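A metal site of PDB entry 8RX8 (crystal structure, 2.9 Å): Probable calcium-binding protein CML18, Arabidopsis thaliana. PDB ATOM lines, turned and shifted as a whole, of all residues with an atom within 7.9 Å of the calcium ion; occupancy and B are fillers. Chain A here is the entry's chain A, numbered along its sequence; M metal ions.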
ATOM      1  N   SER A  35      14.679  12.833  29.801  1.00  0.00           N
ATOM      2  CA  SER A  35      14.596  11.497  29.231  1.00  0.00           C
ATOM      3  C   SER A  35      13.699  10.637  30.100  1.00  0.00           C
ATOM      4  O   SER A  35      13.757  10.710  31.326  1.00  0.00           O
ATOM      5  CB  SER A  35      15.985  10.857  29.088  1.00  0.00           C
ATOM      6  OG  SER A  35      16.710  10.974  30.302  1.00  0.00           O
ATOM      7  N   LEU A  36      12.860   9.835  29.457  1.00  0.00           N
ATOM      8  CA  LEU A  36      11.934   8.955  30.158  1.00  0.00           C
ATOM      9  C   LEU A  36      12.567   7.587  30.384  1.00  0.00           C
ATOM     10  O   LEU A  36      13.258   7.059  29.507  1.00  0.00           O
ATOM     11  CB  LEU A  36      10.619   8.809  29.382  1.00  0.00           C
ATOM     12  CG  LEU A  36       9.484   9.769  29.742  1.00  0.00           C
ATOM     13  CD1 LEU A  36       8.162   9.027  29.772  1.00  0.00           C
ATOM     14  CD2 LEU A  36       9.739  10.470  31.077  1.00  0.00           C
ATOM     15  N   ILE A  61      10.835   0.588  24.034  1.00  0.00           N
ATOM     16  CA  ILE A  61      12.119   1.230  24.305  1.00  0.00           C
ATOM     17  C   ILE A  61      13.111   0.929  23.184  1.00  0.00           C
ATOM     18  O   ILE A  61      13.811   1.831  22.691  1.00  0.00           O
ATOM     19  CB  ILE A  61      12.663   0.787  25.680  1.00  0.00           C
ATOM     20  CG1 ILE A  61      11.901   1.495  26.794  1.00  0.00           C
ATOM     21  CG2 ILE A  61      14.155   1.053  25.785  1.00  0.00           C
ATOM     22  CD1 ILE A  61      12.403   2.880  27.090  1.00  0.00           C
ATOM     23  N   ALA A  64      12.552   2.984  20.104  1.00  0.00           N
ATOM     24  CA  ALA A  64      12.703   4.431  20.195  1.00  0.00           C
ATOM     25  C   ALA A  64      14.123   4.852  20.511  1.00  0.00           C
ATOM     26  O   ALA A  64      14.628   5.804  19.920  1.00  0.00           O
ATOM     27  CB  ALA A  64      11.772   5.004  21.266  1.00  0.00           C
ATOM     28  N   ASP A  65      14.764   4.165  21.449  1.00  0.00           N
ATOM     29  CA  ASP A  65      16.110   4.502  21.891  1.00  0.00           C
ATOM     30  C   ASP A  65      17.075   4.444  20.713  1.00  0.00           C
ATOM     31  O   ASP A  65      17.749   3.434  20.519  1.00  0.00           O
ATOM     32  CB  ASP A  65      16.531   3.547  23.006  1.00  0.00           C
ATOM     33  CG  ASP A  65      17.657   4.072  23.844  1.00  0.00           C
ATOM     34  OD1 ASP A  65      17.666   5.278  24.140  1.00  0.00           O
ATOM     35  OD2 ASP A  65      18.517   3.258  24.257  1.00  0.00           O
ATOM     36  N   ARG A  66      17.165   5.530  19.928  1.00  0.00           N
ATOM     37  CA  ARG A  66      18.040   5.519  18.759  1.00  0.00           C
ATOM     38  C   ARG A  66      19.489   5.763  19.143  1.00  0.00           C
ATOM     39  O   ARG A  66      20.398   5.238  18.500  1.00  0.00           O
ATOM     40  CB  ARG A  66      17.586   6.535  17.720  1.00  0.00           C
ATOM     41  CG  ARG A  66      18.127   6.253  16.320  1.00  0.00           C
ATOM     42  CD  ARG A  66      17.736   7.317  15.294  1.00  0.00           C
ATOM     43  NE  ARG A  66      16.453   7.920  15.570  1.00  0.00           N
ATOM     44  CZ  ARG A  66      15.294   7.581  15.003  1.00  0.00           C
ATOM     45  NH1 ARG A  66      14.924   6.312  14.909  1.00  0.00           N
ATOM     46  NH2 ARG A  66      14.407   8.525  14.739  1.00  0.00           N
ATOM     47  N   ASN A  67      19.718   6.569  20.175  1.00  0.00           N
ATOM     48  CA  ASN A  67      21.067   6.818  20.666  1.00  0.00           C
ATOM     49  C   ASN A  67      21.591   5.665  21.507  1.00  0.00           C
ATOM     50  O   ASN A  67      22.735   5.713  21.958  1.00  0.00           O
ATOM     51  CB  ASN A  67      21.115   8.121  21.458  1.00  0.00           C
ATOM     52  CG  ASN A  67      19.833   8.390  22.210  1.00  0.00           C
ATOM     53  OD1 ASN A  67      19.175   7.470  22.680  1.00  0.00           O
ATOM     54  ND2 ASN A  67      19.469   9.665  22.318  1.00  0.00           N
ATOM     55  N   ASN A  68      20.774   4.626  21.722  1.00  0.00           N
ATOM     56  CA  ASN A  68      21.118   3.487  22.579  1.00  0.00           C
ATOM     57  C   ASN A  68      21.488   3.945  23.988  1.00  0.00           C
ATOM     58  O   ASN A  68      22.244   3.275  24.692  1.00  0.00           O
ATOM     59  CB  ASN A  68      22.225   2.638  21.958  1.00  0.00           C
ATOM     60  CG  ASN A  68      21.914   2.221  20.514  1.00  0.00           C
ATOM     61  OD1 ASN A  68      22.801   1.788  19.787  1.00  0.00           O
ATOM     62  ND2 ASN A  68      20.640   2.308  20.129  1.00  0.00           N
ATOM     63  N   ASN A  69      20.971   5.109  24.376  1.00  0.00           N
ATOM     64  CA  ASN A  69      21.216   5.639  25.718  1.00  0.00           C
ATOM     65  C   ASN A  69      20.673   4.694  26.791  1.00  0.00           C
ATOM     66  O   ASN A  69      21.359   4.390  27.768  1.00  0.00           O
ATOM     67  CB  ASN A  69      20.537   7.006  25.863  1.00  0.00           C
ATOM     68  CG  ASN A  69      21.315   8.121  25.191  1.00  0.00           C
ATOM     69  OD1 ASN A  69      20.844   9.255  25.104  1.00  0.00           O
ATOM     70  ND2 ASN A  69      22.513   7.800  24.713  1.00  0.00           N
ATOM     71  N   GLY A  70      19.443   4.222  26.603  1.00  0.00           N
ATOM     72  CA  GLY A  70      18.734   3.424  27.578  1.00  0.00           C
ATOM     73  C   GLY A  70      17.527   4.135  28.127  1.00  0.00           C
ATOM     74  O   GLY A  70      16.741   3.519  28.867  1.00  0.00           O
ATOM     75  N   LEU A  71      17.349   5.394  27.777  1.00  0.00           N
ATOM     76  CA  LEU A  71      16.211   6.203  28.191  1.00  0.00           C
ATOM     77  C   LEU A  71      15.637   6.852  26.943  1.00  0.00           C
ATOM     78  O   LEU A  71      16.360   7.134  25.985  1.00  0.00           O
ATOM     79  CB  LEU A  71      16.638   7.274  29.205  1.00  0.00           C
ATOM     80  CG  LEU A  71      17.300   6.826  30.497  1.00  0.00           C
ATOM     81  CD1 LEU A  71      17.566   8.008  31.421  1.00  0.00           C
ATOM     82  CD2 LEU A  71      16.469   5.769  31.198  1.00  0.00           C
ATOM     83  N   VAL A  72      14.331   7.100  26.956  1.00  0.00           N
ATOM     84  CA  VAL A  72      13.655   7.689  25.802  1.00  0.00           C
ATOM     85  C   VAL A  72      13.599   9.202  25.983  1.00  0.00           C
ATOM     86  O   VAL A  72      13.049   9.693  26.978  1.00  0.00           O
ATOM     87  CB  VAL A  72      12.254   7.098  25.586  1.00  0.00           C
ATOM     88  CG1 VAL A  72      11.718   6.475  26.871  1.00  0.00           C
ATOM     89  CG2 VAL A  72      11.294   8.138  25.009  1.00  0.00           C
ATOM     90  N   GLU A  73      14.191   9.926  25.052  1.00  0.00           N
ATOM     91  CA  GLU A  73      14.227  11.377  25.081  1.00  0.00           C
ATOM     92  C   GLU A  73      13.070  11.914  24.253  1.00  0.00           C
ATOM     93  O   GLU A  73      12.422  11.185  23.506  1.00  0.00           O
ATOM     94  CB  GLU A  73      15.570  11.890  24.572  1.00  0.00           C
ATOM     95  CG  GLU A  73      16.713  11.694  25.565  1.00  0.00           C
ATOM     96  CD  GLU A  73      17.338  10.312  25.451  1.00  0.00           C
ATOM     97  OE1 GLU A  73      17.468   9.811  24.320  1.00  0.00           O
ATOM     98  OE2 GLU A  73      17.705   9.735  26.494  1.00  0.00           O
ATOM     99  N   PHE A  74      12.785  13.219  24.413  1.00  0.00           N
ATOM    100  CA  PHE A  74      11.617  13.787  23.735  1.00  0.00           C
ATOM    101  C   PHE A  74      11.699  13.595  22.230  1.00  0.00           C
ATOM    102  O   PHE A  74      10.680  13.333  21.575  1.00  0.00           O
ATOM    103  CB  PHE A  74      11.469  15.262  24.080  1.00  0.00           C
ATOM    104  CG  PHE A  74      10.181  15.856  23.614  1.00  0.00           C
ATOM    105  CD1 PHE A  74       8.971  15.326  24.028  1.00  0.00           C
ATOM    106  CD2 PHE A  74      10.166  16.934  22.747  1.00  0.00           C
ATOM    107  CE1 PHE A  74       7.780  15.862  23.587  1.00  0.00           C
ATOM    108  CE2 PHE A  74       8.984  17.484  22.312  1.00  0.00           C
ATOM    109  CZ  PHE A  74       7.778  16.940  22.736  1.00  0.00           C
ATOM    110  N   SER A  75      12.898  13.710  21.659  1.00  0.00           N
ATOM    111  CA  SER A  75      13.047  13.515  20.215  1.00  0.00           C
ATOM    112  C   SER A  75      12.672  12.086  19.829  1.00  0.00           C
ATOM    113  O   SER A  75      11.965  11.882  18.833  1.00  0.00           O
ATOM    114  CB  SER A  75      14.480  13.833  19.776  1.00  0.00           C
ATOM    115  OG  SER A  75      15.429  13.270  20.657  1.00  0.00           O
ATOM    116  N   GLU A  76      13.128  11.094  20.596  1.00  0.00           N
ATOM    117  CA  GLU A  76      12.790   9.708  20.296  1.00  0.00           C
ATOM    118  C   GLU A  76      11.293   9.478  20.427  1.00  0.00           C
ATOM    119  O   GLU A  76      10.692   8.722  19.655  1.00  0.00           O
ATOM    120  CB  GLU A  76      13.550   8.782  21.242  1.00  0.00           C
ATOM    121  CG  GLU A  76      14.920   9.314  21.662  1.00  0.00           C
ATOM    122  CD  GLU A  76      15.891   8.217  22.065  1.00  0.00           C
ATOM    123  OE1 GLU A  76      15.802   7.754  23.219  1.00  0.00           O
ATOM    124  OE2 GLU A  76      16.734   7.827  21.232  1.00  0.00           O
ATOM    125  N   GLU A 137      26.340   7.064  20.788  1.00  0.00           N
ATOM    126  CA  GLU A 137      25.034   7.694  20.633  1.00  0.00           C
ATOM    127  C   GLU A 137      24.734   8.051  19.176  1.00  0.00           C
ATOM    128  O   GLU A 137      23.624   7.818  18.699  1.00  0.00           O
ATOM    129  CB  GLU A 137      24.953   8.942  21.529  1.00  0.00           C
ATOM    130  CG  GLU A 137      24.111  10.074  20.983  1.00  0.00           C
ATOM    131  CD  GLU A 137      24.290  11.355  21.785  1.00  0.00           C
ATOM    132  OE1 GLU A 137      24.771  11.260  22.939  1.00  0.00           O
ATOM    133  OE2 GLU A 137      23.958  12.441  21.264  1.00  0.00           O
ATOM    134  N   SER A 157      18.316  15.268  15.990  1.00  0.00           N
ATOM    135  CA  SER A 157      17.730  14.765  17.236  1.00  0.00           C
ATOM    136  C   SER A 157      18.106  15.653  18.420  1.00  0.00           C
ATOM    137  O   SER A 157      17.288  15.875  19.324  1.00  0.00           O
ATOM    138  CB  SER A 157      18.167  13.319  17.480  1.00  0.00           C
ATOM    139  OG  SER A 157      17.560  12.792  18.641  1.00  0.00           O
HETATM  140 CA    CA M   1      17.743   7.525  24.287  1.00  0.00          CA
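ND2 of Asn 67 is in hydrogen-bond range of OD1 of Asn 69, at 3.1 Å.
N of Arg 66 sits at hydrogen-bond distance from OE2 of Glu 76 (2.7 Å).
The backbone NH (N) of Asn 69 sits at hydrogen-bond distance from the side-chain carboxylate (OD2) of Asp 65, at 3.1 Å.
The backbone NH (N) of Gly 70 lies within hydrogen-bond range of the side-chain carboxylate (OD2) of Asp 65 (2.7 Å).
O of Asp 65 is in hydrogen-bond range of ND2 of Asn 68.
The side-chain carboxylate of Glu 73 sits close to the side-chain amide oxygen of Asn 69 (3.5 Å).
Merely in contact with the calcium ion: Asn 69.
Within 4 Å of the calcium ion: Asp 65, Asn 67, Asn 69, Leu 71, Glu 73 and Glu 76.
OD1 of Asn 67 binds the calcium ion.
The calcium ion is bound by O of Leu 71 (2.2 Å).
OE1 of Glu 76 binds the calcium ion (2.2 Å).
OD1 of Asp 65 is bound to the calcium ion, at 2.3 Å.
The calcium ion is bound by OE1 of Glu 73 (2.3 Å).
The calcium ion has five donor atoms within binding distance.
Slightly farther from the calcium ion lies the side-chain carboxylate (OE2) of Glu 73 (3.1 Å).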
